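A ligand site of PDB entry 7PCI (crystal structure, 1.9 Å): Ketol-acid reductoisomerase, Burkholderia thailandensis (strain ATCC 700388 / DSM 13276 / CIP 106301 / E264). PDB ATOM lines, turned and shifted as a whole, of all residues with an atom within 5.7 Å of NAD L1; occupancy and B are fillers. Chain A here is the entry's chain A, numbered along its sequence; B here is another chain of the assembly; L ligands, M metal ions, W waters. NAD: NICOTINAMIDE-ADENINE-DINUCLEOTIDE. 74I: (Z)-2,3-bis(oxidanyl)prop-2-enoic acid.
OD1 of Asp 88 sits at hydrogen-bond distance from O3D of NAD L1, 2.6 Å away.
The side-chain amide oxygen (OD1) of Asn 53 is in hydrogen-bond range of an oxygen (O3B) of NAD L1, at 2.7 Å.
O2B of NAD L1 sits at hydrogen-bond distance from OD2 of Asp 56 (2.7 Å).
The backbone NH (N) of Tyr 31 is in hydrogen-bond range of an oxygen (O3B) of NAD L1, 2.8 Å away.
The backbone NH of Gln 34 lies within hydrogen-bond range of an oxygen (O2N) of NAD L1 (3.0 Å).
The side-chain amide nitrogen (NE2) of Gln 34 sits close to an oxygen (O7N) of NAD L1 (3.5 Å).
The backbone NH of Ile 33 is in hydrogen-bond range of an oxygen (O2A) of NAD L1 (3.0 Å).
The backbone carbonyl oxygen (O) of Gln 257 of chain B lies within hydrogen-bond range of a nitrogen (N7N) of NAD L1, at 3.3 Å.
The backbone NH of Ser 259 of chain B sits at hydrogen-bond distance from an oxygen (O3) of 74I L2 (3.0 Å).
OG of Ser 259 of chain B lies close to O2 of 74I L2.
OE2 of Glu 237 of chain B lies close to O7 of 74I L2 (2.5 Å).
The side-chain carboxylate (OD2) of Asp 88 sits at hydrogen-bond distance from the side-chain hydroxyl (OG1) of Thr 261 of chain B (2.8 Å).
The side-chain carboxylate of Asp 56 sits at hydrogen-bond distance from the side-chain amide nitrogen of Asn 53 (2.9 Å).
The side-chain amide oxygen (OD1) of Asn 53 lies within hydrogen-bond range of the backbone NH (N) of Tyr 31, at 3.2 Å.
NE2 of Gln 34 sits at hydrogen-bond distance from O of Met 137.
The side-chain amide oxygen of Gln 257 of chain B sits at hydrogen-bond distance from the backbone NH of Gly 139 (3.1 Å).
N of Thr 261 of chain B sits close to OG of Ser 259 of chain B (3.5 Å).
NE2 of His 91 sits at hydrogen-bond distance from O of Ile 86 (2.8 Å).
The backbone carbonyl oxygen (O) of Ile 29 sits at hydrogen-bond distance from the backbone NH (N) of Leu 85 (2.7 Å).
A nitrogen (N7N) of NAD L1 lies close to an oxygen (O3) of 74I L2.
Water W3 lies within hydrogen-bond range of an oxygen (O2A) of NAD L1 and the side-chain hydroxyl (OH) of Tyr 58.
Water W7 lies within hydrogen-bond range of the backbone carbonyl oxygen of Leu 84 (2.6 Å), an oxygen (O3D) of NAD L1 (2.7 Å) and the backbone NH of Ala 112 (2.8 Å).
Water W1 lies within hydrogen-bond range of O of Leu 85 (2.6 Å), O2N of NAD L1 (2.8 Å), N of Gly 35 (2.9 Å) and N of Gly 32 (3.0 Å).
Water W6 lies within hydrogen-bond range of N3A of NAD L1 (2.8 Å), N of Ile 54 (3.0 Å) and ND2 of Asn 53 (3.4 Å).
Water W5 lies within hydrogen-bond range of O of Ala 112 and ND1 of His 113.
N of Ser 259 of chain B sits close to N7N of NAD L1, 3.5 Å away.
Merely in contact with NAD L1: Gly 30 (3.2 Å), Gly 32 (3.3 Å), Ile 54 (3.5 Å), Tyr 58 (3.3 Å), Leu 85 (3.6 Å), Ile 86 (3.3 Å), Pro 87 (3.3 Å), Ala 90 (3.5 Å), His 91 (3.6 Å), Val 94 (3.7 Å), Ala 112 (3.4 Å), His 113 (3.3 Å), Pro 135 (3.9 Å), Met 137 (3.8 Å), Tyr 138 (3.2 Å) and Pro 260 of chain B (3.1 Å).
Hydrophobic or aromatic side chains within 4 Å of NAD L1: Ile 33, Ile 54, Tyr 58, Ile 86, Pro 87, Ala 90, His 91, Val 94, Ala 112, His 113, Tyr 138 and Pro 260 of chain B.
Of the 34 residues printed, 24 come within 4 Å of NAD L1.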
ATOM      1  N   ILE A  29       1.656 -22.138  -8.177  1.00  0.00           N
ATOM      2  CA  ILE A  29       2.479 -23.264  -8.702  1.00  0.00           C
ATOM      3  C   ILE A  29       2.193 -23.391 -10.198  1.00  0.00           C
ATOM      4  O   ILE A  29       1.052 -23.749 -10.548  1.00  0.00           O
ATOM      5  CB  ILE A  29       2.187 -24.574  -7.937  1.00  0.00           C
ATOM      6  CG1 ILE A  29       2.326 -24.379  -6.423  1.00  0.00           C
ATOM      7  CG2 ILE A  29       3.091 -25.697  -8.442  1.00  0.00           C
ATOM      8  CD1 ILE A  29       3.618 -23.712  -5.986  1.00  0.00           C
ATOM      9  N   GLY A  30       3.209 -23.131 -11.017  1.00  0.00           N
ATOM     10  CA  GLY A  30       3.093 -22.981 -12.478  1.00  0.00           C
ATOM     11  C   GLY A  30       2.900 -21.519 -12.851  1.00  0.00           C
ATOM     12  O   GLY A  30       2.312 -20.777 -12.047  1.00  0.00           O
ATOM     13  N   TYR A  31       3.396 -21.120 -14.020  1.00  0.00           N
ATOM     14  CA  TYR A  31       3.322 -19.724 -14.519  1.00  0.00           C
ATOM     15  C   TYR A  31       2.924 -19.753 -15.992  1.00  0.00           C
ATOM     16  O   TYR A  31       3.451 -18.977 -16.799  1.00  0.00           O
ATOM     17  CB  TYR A  31       4.648 -19.007 -14.252  1.00  0.00           C
ATOM     18  CG  TYR A  31       4.557 -17.502 -14.324  1.00  0.00           C
ATOM     19  CD1 TYR A  31       4.020 -16.772 -13.284  1.00  0.00           C
ATOM     20  CD2 TYR A  31       5.017 -16.820 -15.431  1.00  0.00           C
ATOM     21  CE1 TYR A  31       3.940 -15.387 -13.339  1.00  0.00           C
ATOM     22  CE2 TYR A  31       4.950 -15.434 -15.501  1.00  0.00           C
ATOM     23  CZ  TYR A  31       4.402 -14.718 -14.444  1.00  0.00           C
ATOM     24  OH  TYR A  31       4.328 -13.349 -14.522  1.00  0.00           O
ATOM     25  N   GLY A  32       1.989 -20.664 -16.316  1.00  0.00           N
ATOM     26  CA  GLY A  32       1.443 -20.823 -17.673  1.00  0.00           C
ATOM     27  C   GLY A  32       0.262 -19.896 -17.897  1.00  0.00           C
ATOM     28  O   GLY A  32       0.263 -18.769 -17.360  1.00  0.00           O
ATOM     29  N   ILE A  33      -0.727 -20.377 -18.644  1.00  0.00           N
ATOM     30  CA  ILE A  33      -1.899 -19.597 -19.127  1.00  0.00           C
ATOM     31  C   ILE A  33      -2.644 -19.036 -17.905  1.00  0.00           C
ATOM     32  O   ILE A  33      -2.903 -17.812 -17.875  1.00  0.00           O
ATOM     33  CB  ILE A  33      -2.791 -20.471 -20.037  1.00  0.00           C
ATOM     34  CG1 ILE A  33      -2.037 -20.911 -21.298  1.00  0.00           C
ATOM     35  CG2 ILE A  33      -4.089 -19.770 -20.381  1.00  0.00           C
ATOM     36  CD1 ILE A  33      -2.446 -22.265 -21.855  1.00  0.00           C
ATOM     37  N   GLN A  34      -2.946 -19.885 -16.921  1.00  0.00           N
ATOM     38  CA  GLN A  34      -3.693 -19.513 -15.698  1.00  0.00           C
ATOM     39  C   GLN A  34      -2.732 -18.929 -14.658  1.00  0.00           C
ATOM     40  O   GLN A  34      -3.026 -17.826 -14.149  1.00  0.00           O
ATOM     41  CB  GLN A  34      -4.448 -20.722 -15.151  1.00  0.00           C
ATOM     42  CG  GLN A  34      -5.658 -21.111 -15.989  1.00  0.00           C
ATOM     43  CD  GLN A  34      -6.739 -20.052 -15.951  1.00  0.00           C
ATOM     44  OE1 GLN A  34      -7.029 -19.497 -14.895  1.00  0.00           O
ATOM     45  NE2 GLN A  34      -7.340 -19.767 -17.089  1.00  0.00           N
ATOM     46  N   GLY A  35      -1.631 -19.624 -14.373  1.00  0.00           N
ATOM     47  CA  GLY A  35      -0.642 -19.224 -13.344  1.00  0.00           C
ATOM     48  C   GLY A  35      -0.217 -17.776 -13.502  1.00  0.00           C
ATOM     49  O   GLY A  35      -0.168 -17.058 -12.479  1.00  0.00           O
ATOM     50  N   ASN A  53       7.879 -23.066  -9.645  1.00  0.00           N
ATOM     51  CA  ASN A  53       7.964 -23.510 -11.061  1.00  0.00           C
ATOM     52  C   ASN A  53       9.228 -24.351 -11.260  1.00  0.00           C
ATOM     53  O   ASN A  53      10.254 -24.031 -10.637  1.00  0.00           O
ATOM     54  CB  ASN A  53       7.916 -22.311 -12.010  1.00  0.00           C
ATOM     55  CG  ASN A  53       7.464 -22.668 -13.412  1.00  0.00           C
ATOM     56  OD1 ASN A  53       6.330 -22.390 -13.790  1.00  0.00           O
ATOM     57  ND2 ASN A  53       8.341 -23.278 -14.187  1.00  0.00           N
ATOM     58  N   ILE A  54       9.127 -25.401 -12.076  1.00  0.00           N
ATOM     59  CA  ILE A  54      10.269 -26.253 -12.523  1.00  0.00           C
ATOM     60  C   ILE A  54      11.218 -25.393 -13.373  1.00  0.00           C
ATOM     61  O   ILE A  54      10.812 -24.282 -13.785  1.00  0.00           O
ATOM     62  CB  ILE A  54       9.788 -27.502 -13.292  1.00  0.00           C
ATOM     63  CG1 ILE A  54       9.086 -27.141 -14.602  1.00  0.00           C
ATOM     64  CG2 ILE A  54       8.925 -28.375 -12.391  1.00  0.00           C
ATOM     65  CD1 ILE A  54       8.642 -28.326 -15.442  1.00  0.00           C
ATOM     66  N   ASP A  56      12.255 -24.369 -16.352  1.00  0.00           N
ATOM     67  CA  ASP A  56      11.877 -24.237 -17.783  1.00  0.00           C
ATOM     68  C   ASP A  56      11.649 -22.747 -18.106  1.00  0.00           C
ATOM     69  O   ASP A  56      11.919 -21.917 -17.228  1.00  0.00           O
ATOM     70  CB  ASP A  56      10.664 -25.115 -18.118  1.00  0.00           C
ATOM     71  CG  ASP A  56       9.384 -24.722 -17.414  1.00  0.00           C
ATOM     72  OD1 ASP A  56       9.341 -23.601 -16.849  1.00  0.00           O
ATOM     73  OD2 ASP A  56       8.431 -25.526 -17.436  1.00  0.00           O
ATOM     74  N   TYR A  58       9.101 -20.852 -18.287  1.00  0.00           N
ATOM     75  CA  TYR A  58       8.087 -20.166 -17.445  1.00  0.00           C
ATOM     76  C   TYR A  58       8.737 -19.593 -16.188  1.00  0.00           C
ATOM     77  O   TYR A  58       8.306 -18.521 -15.712  1.00  0.00           O
ATOM     78  CB  TYR A  58       6.952 -21.140 -17.100  1.00  0.00           C
ATOM     79  CG  TYR A  58       6.180 -21.655 -18.289  1.00  0.00           C
ATOM     80  CD1 TYR A  58       6.477 -22.894 -18.842  1.00  0.00           C
ATOM     81  CD2 TYR A  58       5.140 -20.924 -18.843  1.00  0.00           C
ATOM     82  CE1 TYR A  58       5.765 -23.391 -19.921  1.00  0.00           C
ATOM     83  CE2 TYR A  58       4.425 -21.408 -19.923  1.00  0.00           C
ATOM     84  CZ  TYR A  58       4.732 -22.643 -20.467  1.00  0.00           C
ATOM     85  OH  TYR A  58       4.027 -23.129 -21.524  1.00  0.00           O
ATOM     86  N   ILE A  72       9.170 -25.613  -6.831  1.00  0.00           N
ATOM     87  CA  ILE A  72       7.778 -25.790  -6.328  1.00  0.00           C
ATOM     88  C   ILE A  72       7.822 -26.049  -4.817  1.00  0.00           C
ATOM     89  O   ILE A  72       6.981 -25.462  -4.105  1.00  0.00           O
ATOM     90  CB  ILE A  72       7.056 -26.905  -7.107  1.00  0.00           C
ATOM     91  CG1 ILE A  72       6.907 -26.531  -8.587  1.00  0.00           C
ATOM     92  CG2 ILE A  72       5.722 -27.225  -6.449  1.00  0.00           C
ATOM     93  CD1 ILE A  72       6.315 -27.612  -9.463  1.00  0.00           C
ATOM     94  N   LEU A  84      -2.432 -24.770  -7.539  1.00  0.00           N
ATOM     95  CA  LEU A  84      -1.795 -25.769  -8.448  1.00  0.00           C
ATOM     96  C   LEU A  84      -2.251 -25.515  -9.890  1.00  0.00           C
ATOM     97  O   LEU A  84      -3.262 -26.112 -10.310  1.00  0.00           O
ATOM     98  CB  LEU A  84      -2.165 -27.176  -7.991  1.00  0.00           C
ATOM     99  CG  LEU A  84      -1.510 -28.315  -8.768  1.00  0.00           C
ATOM    100  CD1 LEU A  84      -0.011 -28.083  -8.925  1.00  0.00           C
ATOM    101  CD2 LEU A  84      -1.765 -29.659  -8.094  1.00  0.00           C
ATOM    102  N   LEU A  85      -1.527 -24.653 -10.606  1.00  0.00           N
ATOM    103  CA  LEU A  85      -1.880 -24.190 -11.983  1.00  0.00           C
ATOM    104  C   LEU A  85      -0.830 -24.734 -12.963  1.00  0.00           C
ATOM    105  O   LEU A  85      -0.147 -23.938 -13.626  1.00  0.00           O
ATOM    106  CB  LEU A  85      -1.974 -22.662 -11.976  1.00  0.00           C
ATOM    107  CG  LEU A  85      -3.002 -22.083 -10.988  1.00  0.00           C
ATOM    108  CD1 LEU A  85      -3.005 -20.564 -11.020  1.00  0.00           C
ATOM    109  CD2 LEU A  85      -4.395 -22.612 -11.267  1.00  0.00           C
ATOM    110  N   ILE A  86      -0.746 -26.062 -13.037  1.00  0.00           N
ATOM    111  CA  ILE A  86       0.057 -26.831 -14.040  1.00  0.00           C
ATOM    112  C   ILE A  86      -0.894 -27.819 -14.724  1.00  0.00           C
ATOM    113  O   ILE A  86      -2.004 -28.030 -14.234  1.00  0.00           O
ATOM    114  CB  ILE A  86       1.264 -27.529 -13.357  1.00  0.00           C
ATOM    115  CG1 ILE A  86       0.821 -28.694 -12.479  1.00  0.00           C
ATOM    116  CG2 ILE A  86       2.098 -26.517 -12.589  1.00  0.00           C
ATOM    117  CD1 ILE A  86       1.959 -29.540 -11.950  1.00  0.00           C
ATOM    118  N   PRO A  87      -0.517 -28.433 -15.865  1.00  0.00           N
ATOM    119  CA  PRO A  87      -1.398 -29.379 -16.551  1.00  0.00           C
ATOM    120  C   PRO A  87      -1.857 -30.520 -15.632  1.00  0.00           C
ATOM    121  O   PRO A  87      -1.091 -30.981 -14.813  1.00  0.00           O
ATOM    122  CB  PRO A  87      -0.539 -29.902 -17.706  1.00  0.00           C
ATOM    123  CG  PRO A  87       0.429 -28.776 -17.965  1.00  0.00           C
ATOM    124  CD  PRO A  87       0.743 -28.224 -16.598  1.00  0.00           C
ATOM    125  N   ASP A  88      -3.101 -30.960 -15.836  1.00  0.00           N
ATOM    126  CA  ASP A  88      -3.868 -31.849 -14.916  1.00  0.00           C
ATOM    127  C   ASP A  88      -3.167 -33.207 -14.790  1.00  0.00           C
ATOM    128  O   ASP A  88      -3.158 -33.746 -13.667  1.00  0.00           O
ATOM    129  CB  ASP A  88      -5.310 -31.969 -15.395  1.00  0.00           C
ATOM    130  CG  ASP A  88      -5.995 -30.619 -15.493  1.00  0.00           C
ATOM    131  OD1 ASP A  88      -6.335 -30.063 -14.416  1.00  0.00           O
ATOM    132  OD2 ASP A  88      -6.135 -30.105 -16.616  1.00  0.00           O
ATOM    133  N   ALA A  90      -0.076 -33.826 -14.762  1.00  0.00           N
ATOM    134  CA  ALA A  90       1.160 -33.618 -13.964  1.00  0.00           C
ATOM    135  C   ALA A  90       0.833 -33.458 -12.473  1.00  0.00           C
ATOM    136  O   ALA A  90       1.784 -33.485 -11.665  1.00  0.00           O
ATOM    137  CB  ALA A  90       1.917 -32.429 -14.497  1.00  0.00           C
ATOM    138  N   HIS A  91      -0.431 -33.286 -12.106  1.00  0.00           N
ATOM    139  CA  HIS A  91      -0.890 -32.997 -10.717  1.00  0.00           C
ATOM    140  C   HIS A  91      -0.444 -34.112  -9.764  1.00  0.00           C
ATOM    141  O   HIS A  91       0.097 -33.786  -8.690  1.00  0.00           O
ATOM    142  CB  HIS A  91      -2.407 -32.802 -10.649  1.00  0.00           C
ATOM    143  CG  HIS A  91      -2.882 -31.493 -11.169  1.00  0.00           C
ATOM    144  ND1 HIS A  91      -4.120 -30.983 -10.867  1.00  0.00           N
ATOM    145  CD2 HIS A  91      -2.279 -30.577 -11.966  1.00  0.00           C
ATOM    146  CE1 HIS A  91      -4.274 -29.809 -11.452  1.00  0.00           C
ATOM    147  NE2 HIS A  91      -3.152 -29.540 -12.132  1.00  0.00           N
ATOM    148  N   VAL A  94       3.417 -34.137  -8.899  1.00  0.00           N
ATOM    149  CA  VAL A  94       3.784 -32.856  -8.221  1.00  0.00           C
ATOM    150  C   VAL A  94       3.132 -32.815  -6.831  1.00  0.00           C
ATOM    151  O   VAL A  94       3.774 -32.291  -5.898  1.00  0.00           O
ATOM    152  CB  VAL A  94       3.395 -31.623  -9.073  1.00  0.00           C
ATOM    153  CG1 VAL A  94       3.502 -30.322  -8.293  1.00  0.00           C
ATOM    154  CG2 VAL A  94       4.230 -31.563 -10.342  1.00  0.00           C
ATOM    155  N   ALA A 112      -7.731 -25.560 -10.320  1.00  0.00           N
ATOM    156  CA  ALA A 112      -8.586 -24.725 -11.201  1.00  0.00           C
ATOM    157  C   ALA A 112      -9.412 -25.618 -12.133  1.00  0.00           C
ATOM    158  O   ALA A 112     -10.023 -25.085 -13.077  1.00  0.00           O
ATOM    159  CB  ALA A 112      -7.732 -23.742 -11.968  1.00  0.00           C
ATOM    160  N   HIS A 113      -9.448 -26.925 -11.853  1.00  0.00           N
ATOM    161  CA  HIS A 113     -10.166 -27.962 -12.652  1.00  0.00           C
ATOM    162  C   HIS A 113     -10.286 -29.218 -11.780  1.00  0.00           C
ATOM    163  O   HIS A 113      -9.324 -29.513 -11.044  1.00  0.00           O
ATOM    164  CB  HIS A 113      -9.430 -28.183 -13.987  1.00  0.00           C
ATOM    165  CG  HIS A 113     -10.074 -29.163 -14.905  1.00  0.00           C
ATOM    166  ND1 HIS A 113     -11.430 -29.173 -15.162  1.00  0.00           N
ATOM    167  CD2 HIS A 113      -9.542 -30.149 -15.664  1.00  0.00           C
ATOM    168  CE1 HIS A 113     -11.716 -30.135 -16.022  1.00  0.00           C
ATOM    169  NE2 HIS A 113     -10.574 -30.746 -16.348  1.00  0.00           N
ATOM    170  N   ALA A 134     -12.347 -22.713 -10.318  1.00  0.00           N
ATOM    171  CA  ALA A 134     -12.229 -23.017 -11.763  1.00  0.00           C
ATOM    172  C   ALA A 134     -12.794 -21.848 -12.564  1.00  0.00           C
ATOM    173  O   ALA A 134     -14.014 -21.696 -12.660  1.00  0.00           O
ATOM    174  CB  ALA A 134     -12.955 -24.312 -12.065  1.00  0.00           C
ATOM    175  N   PRO A 135     -11.939 -20.981 -13.158  1.00  0.00           N
ATOM    176  CA  PRO A 135     -12.403 -19.876 -13.992  1.00  0.00           C
ATOM    177  C   PRO A 135     -13.138 -20.392 -15.242  1.00  0.00           C
ATOM    178  O   PRO A 135     -12.728 -21.423 -15.762  1.00  0.00           O
ATOM    179  CB  PRO A 135     -11.112 -19.139 -14.382  1.00  0.00           C
ATOM    180  CG  PRO A 135     -10.130 -19.557 -13.320  1.00  0.00           C
ATOM    181  CD  PRO A 135     -10.472 -21.005 -13.059  1.00  0.00           C
ATOM    182  N   MET A 137     -13.085 -19.083 -18.188  1.00  0.00           N
ATOM    183  CA  MET A 137     -12.336 -18.151 -19.082  1.00  0.00           C
ATOM    184  C   MET A 137     -10.868 -18.567 -19.110  1.00  0.00           C
ATOM    185  O   MET A 137     -10.421 -19.191 -18.119  1.00  0.00           O
ATOM    186  CB  MET A 137     -12.457 -16.715 -18.560  1.00  0.00           C
ATOM    187  CG  MET A 137     -11.981 -15.650 -19.535  1.00  0.00           C
ATOM    188  SD  MET A 137     -12.834 -15.710 -21.129  1.00  0.00           S
ATOM    189  CE  MET A 137     -14.514 -15.338 -20.617  1.00  0.00           C
ATOM    190  N   TYR A 138     -10.156 -18.254 -20.194  1.00  0.00           N
ATOM    191  CA  TYR A 138      -8.706 -18.537 -20.342  1.00  0.00           C
ATOM    192  C   TYR A 138      -7.914 -17.299 -19.900  1.00  0.00           C
ATOM    193  O   TYR A 138      -8.522 -16.258 -19.575  1.00  0.00           O
ATOM    194  CB  TYR A 138      -8.368 -19.062 -21.746  1.00  0.00           C
ATOM    195  CG  TYR A 138      -8.909 -18.298 -22.926  1.00  0.00           C
ATOM    196  CD1 TYR A 138      -8.161 -17.319 -23.560  1.00  0.00           C
ATOM    197  CD2 TYR A 138     -10.152 -18.598 -23.463  1.00  0.00           C
ATOM    198  CE1 TYR A 138      -8.629 -16.634 -24.664  1.00  0.00           C
ATOM    199  CE2 TYR A 138     -10.641 -17.924 -24.573  1.00  0.00           C
ATOM    200  CZ  TYR A 138      -9.879 -16.939 -25.180  1.00  0.00           C
ATOM    201  OH  TYR A 138     -10.350 -16.282 -26.274  1.00  0.00           O
ATOM    202  N   GLY A 139      -6.579 -17.428 -19.859  1.00  0.00           N
ATOM    203  CA  GLY A 139      -5.642 -16.558 -19.112  1.00  0.00           C
ATOM    204  C   GLY A 139      -5.697 -15.098 -19.535  1.00  0.00           C
ATOM    205  O   GLY A 139      -5.907 -14.251 -18.650  1.00  0.00           O
ATOM    206  N   ASP A 196     -16.601 -28.894 -18.232  1.00  0.00           N
ATOM    207  CA  ASP A 196     -15.396 -28.256 -18.815  1.00  0.00           C
ATOM    208  C   ASP A 196     -14.927 -29.071 -20.019  1.00  0.00           C
ATOM    209  O   ASP A 196     -14.740 -28.495 -21.096  1.00  0.00           O
ATOM    210  CB  ASP A 196     -14.284 -28.143 -17.770  1.00  0.00           C
ATOM    211  CG  ASP A 196     -13.227 -27.128 -18.130  1.00  0.00           C
ATOM    212  OD1 ASP A 196     -13.599 -25.946 -18.315  1.00  0.00           O
ATOM    213  OD2 ASP A 196     -12.053 -27.510 -18.237  1.00  0.00           O
ATOM    214  N   GLU B 237     -16.736 -16.984 -22.917  1.00  0.00           N
ATOM    215  CA  GLU B 237     -15.478 -17.712 -23.253  1.00  0.00           C
ATOM    216  C   GLU B 237     -15.500 -18.155 -24.725  1.00  0.00           C
ATOM    217  O   GLU B 237     -14.472 -17.982 -25.389  1.00  0.00           O
ATOM    218  CB  GLU B 237     -15.280 -18.924 -22.343  1.00  0.00           C
ATOM    219  CG  GLU B 237     -13.942 -19.617 -22.575  1.00  0.00           C
ATOM    220  CD  GLU B 237     -13.577 -20.667 -21.557  1.00  0.00           C
ATOM    221  OE1 GLU B 237     -14.491 -21.385 -21.077  1.00  0.00           O
ATOM    222  OE2 GLU B 237     -12.374 -20.780 -21.244  1.00  0.00           O
ATOM    223  N   GLN B 257      -3.785 -20.749 -25.707  1.00  0.00           N
ATOM    224  CA  GLN B 257      -4.504 -20.418 -24.447  1.00  0.00           C
ATOM    225  C   GLN B 257      -5.256 -21.630 -23.871  1.00  0.00           C
ATOM    226  O   GLN B 257      -5.819 -21.476 -22.761  1.00  0.00           O
ATOM    227  CB  GLN B 257      -5.456 -19.239 -24.692  1.00  0.00           C
ATOM    228  CG  GLN B 257      -4.721 -17.903 -24.773  1.00  0.00           C
ATOM    229  CD  GLN B 257      -4.224 -17.449 -23.419  1.00  0.00           C
ATOM    230  OE1 GLN B 257      -4.994 -17.213 -22.497  1.00  0.00           O
ATOM    231  NE2 GLN B 257      -2.917 -17.319 -23.296  1.00  0.00           N
ATOM    232  N   GLY B 258      -5.259 -22.769 -24.560  1.00  0.00           N
ATOM    233  CA  GLY B 258      -5.829 -24.025 -24.035  1.00  0.00           C
ATOM    234  C   GLY B 258      -4.821 -24.783 -23.185  1.00  0.00           C
ATOM    235  O   GLY B 258      -3.658 -24.865 -23.601  1.00  0.00           O
ATOM    236  N   SER B 259      -5.257 -25.318 -22.036  1.00  0.00           N
ATOM    237  CA  SER B 259      -4.484 -26.286 -21.225  1.00  0.00           C
ATOM    238  C   SER B 259      -4.237 -27.535 -22.070  1.00  0.00           C
ATOM    239  O   SER B 259      -5.015 -27.821 -22.980  1.00  0.00           O
ATOM    240  CB  SER B 259      -5.200 -26.641 -19.943  1.00  0.00           C
ATOM    241  OG  SER B 259      -6.227 -27.587 -20.178  1.00  0.00           O
ATOM    242  N   PRO B 260      -3.160 -28.325 -21.812  1.00  0.00           N
ATOM    243  CA  PRO B 260      -2.952 -29.579 -22.530  1.00  0.00           C
ATOM    244  C   PRO B 260      -4.206 -30.477 -22.550  1.00  0.00           C
ATOM    245  O   PRO B 260      -4.479 -31.058 -23.581  1.00  0.00           O
ATOM    246  CB  PRO B 260      -1.810 -30.225 -21.742  1.00  0.00           C
ATOM    247  CG  PRO B 260      -1.008 -29.042 -21.239  1.00  0.00           C
ATOM    248  CD  PRO B 260      -2.069 -28.025 -20.871  1.00  0.00           C
ATOM    249  N   THR B 261      -4.933 -30.541 -21.426  1.00  0.00           N
ATOM    250  CA  THR B 261      -6.206 -31.305 -21.280  1.00  0.00           C
ATOM    251  C   THR B 261      -7.221 -30.804 -22.313  1.00  0.00           C
ATOM    252  O   THR B 261      -7.811 -31.652 -23.025  1.00  0.00           O
ATOM    253  CB  THR B 261      -6.754 -31.188 -19.846  1.00  0.00           C
ATOM    254  OG1 THR B 261      -5.759 -31.675 -18.953  1.00  0.00           O
ATOM    255  CG2 THR B 261      -8.050 -31.951 -19.653  1.00  0.00           C
HETATM  256  PA  NAD L   1      -0.218 -24.636 -19.080  1.00  0.00           P
HETATM  257  O1A NAD L   1      -0.201 -25.592 -20.190  1.00  0.00           O
HETATM  258  O2A NAD L   1      -0.006 -23.212 -19.395  1.00  0.00           O
HETATM  259  O5B NAD L   1       0.836 -25.083 -18.021  1.00  0.00           O
HETATM  260  C5B NAD L   1       2.231 -24.692 -18.143  1.00  0.00           C
HETATM  261  C4B NAD L   1       2.822 -24.506 -16.758  1.00  0.00           C
HETATM  262  O4B NAD L   1       2.847 -25.773 -16.079  1.00  0.00           O
HETATM  263  C3B NAD L   1       4.254 -23.976 -16.647  1.00  0.00           C
HETATM  264  O3B NAD L   1       4.397 -23.286 -15.417  1.00  0.00           O
HETATM  265  C2B NAD L   1       5.073 -25.256 -16.545  1.00  0.00           C
HETATM  266  O2B NAD L   1       6.274 -25.158 -15.812  1.00  0.00           O
HETATM  267  C1B NAD L   1       4.145 -26.104 -15.689  1.00  0.00           C
HETATM  268  N9A NAD L   1       4.339 -27.526 -15.870  1.00  0.00           N
HETATM  269  C8A NAD L   1       4.069 -28.223 -17.015  1.00  0.00           C
HETATM  270  N7A NAD L   1       4.307 -29.496 -16.889  1.00  0.00           N
HETATM  271  C5A NAD L   1       4.792 -29.649 -15.619  1.00  0.00           C
HETATM  272  C6A NAD L   1       5.242 -30.756 -14.894  1.00  0.00           C
HETATM  273  N6A NAD L   1       5.309 -31.980 -15.387  1.00  0.00           N
HETATM  274  N1A NAD L   1       5.667 -30.560 -13.633  1.00  0.00           N
HETATM  275  C2A NAD L   1       5.645 -29.314 -13.153  1.00  0.00           C
HETATM  276  N3A NAD L   1       5.224 -28.205 -13.728  1.00  0.00           N
HETATM  277  C4A NAD L   1       4.820 -28.431 -14.971  1.00  0.00           C
HETATM  278  O3  NAD L   1      -1.543 -24.863 -18.272  1.00  0.00           O
HETATM  279  PN  NAD L   1      -2.856 -24.101 -17.931  1.00  0.00           P
HETATM  280  O1N NAD L   1      -3.670 -23.974 -19.139  1.00  0.00           O
HETATM  281  O2N NAD L   1      -2.456 -22.841 -17.238  1.00  0.00           O
HETATM  282  O5D NAD L   1      -3.558 -25.074 -16.915  1.00  0.00           O
HETATM  283  C5D NAD L   1      -3.349 -24.980 -15.505  1.00  0.00           C
HETATM  284  C4D NAD L   1      -4.520 -25.547 -14.750  1.00  0.00           C
HETATM  285  O4D NAD L   1      -5.649 -24.694 -14.889  1.00  0.00           O
HETATM  286  C3D NAD L   1      -5.012 -26.950 -15.169  1.00  0.00           C
HETATM  287  O3D NAD L   1      -5.487 -27.592 -14.007  1.00  0.00           O
HETATM  288  C2D NAD L   1      -6.177 -26.600 -16.089  1.00  0.00           C
HETATM  289  O2D NAD L   1      -7.115 -27.637 -16.261  1.00  0.00           O
HETATM  290  C1D NAD L   1      -6.732 -25.350 -15.392  1.00  0.00           C
HETATM  291  N1N NAD L   1      -7.445 -24.417 -16.287  1.00  0.00           N
HETATM  292  C2N NAD L   1      -6.794 -23.835 -17.331  1.00  0.00           C
HETATM  293  C3N NAD L   1      -7.463 -22.940 -18.133  1.00  0.00           C
HETATM  294  C7N NAD L   1      -6.829 -22.386 -19.383  1.00  0.00           C
HETATM  295  O7N NAD L   1      -7.453 -21.582 -20.054  1.00  0.00           O
HETATM  296  N7N NAD L   1      -5.622 -22.784 -19.721  1.00  0.00           N
HETATM  297  C4N NAD L   1      -8.716 -22.534 -17.770  1.00  0.00           C
HETATM  298  C5N NAD L   1      -9.320 -23.103 -16.695  1.00  0.00           C
HETATM  299  C6N NAD L   1      -8.688 -24.109 -16.029  1.00  0.00           C
HETATM  300  C4  74I L   2     -10.087 -24.397 -19.814  1.00  0.00           C
HETATM  301  C5  74I L   2     -10.472 -22.964 -20.175  1.00  0.00           C
HETATM  302  O3  74I L   2      -7.996 -24.453 -21.047  1.00  0.00           O
HETATM  303  C1  74I L   2      -8.809 -25.069 -20.317  1.00  0.00           C
HETATM  304  O2  74I L   2      -8.575 -26.251 -19.973  1.00  0.00           O
HETATM  305  O6  74I L   2     -10.925 -25.121 -19.032  1.00  0.00           O
HETATM  306  O7  74I L   2     -11.657 -22.501 -19.637  1.00  0.00           O
HETATM  307 MG    MG M   1     -10.259 -27.283 -18.898  1.00  0.00          MG
HETATM  308 MG    MG M   2     -12.970 -24.261 -18.981  1.00  0.00          MG
HETATM  309  O   HOH W   1      -0.480 -22.064 -15.469  1.00  0.00           O
HETATM  310  O   HOH W   2       2.926 -31.165 -18.701  1.00  0.00           O
HETATM  311  O   HOH W   3       1.266 -22.371 -21.526  1.00  0.00           O
HETATM  312  O   HOH W   4     -12.675 -23.684 -16.976  1.00  0.00           O
HETATM  313  O   HOH W   5     -11.518 -25.739 -15.240  1.00  0.00           O
HETATM  314  O   HOH W   6       6.323 -25.714 -13.032  1.00  0.00           O
HETATM  315  O   HOH W   7      -5.496 -26.755 -11.425  1.00  0.00           O
HETATM  316  O   HOH W   8      -9.690 -26.816 -17.096  1.00  0.00           O
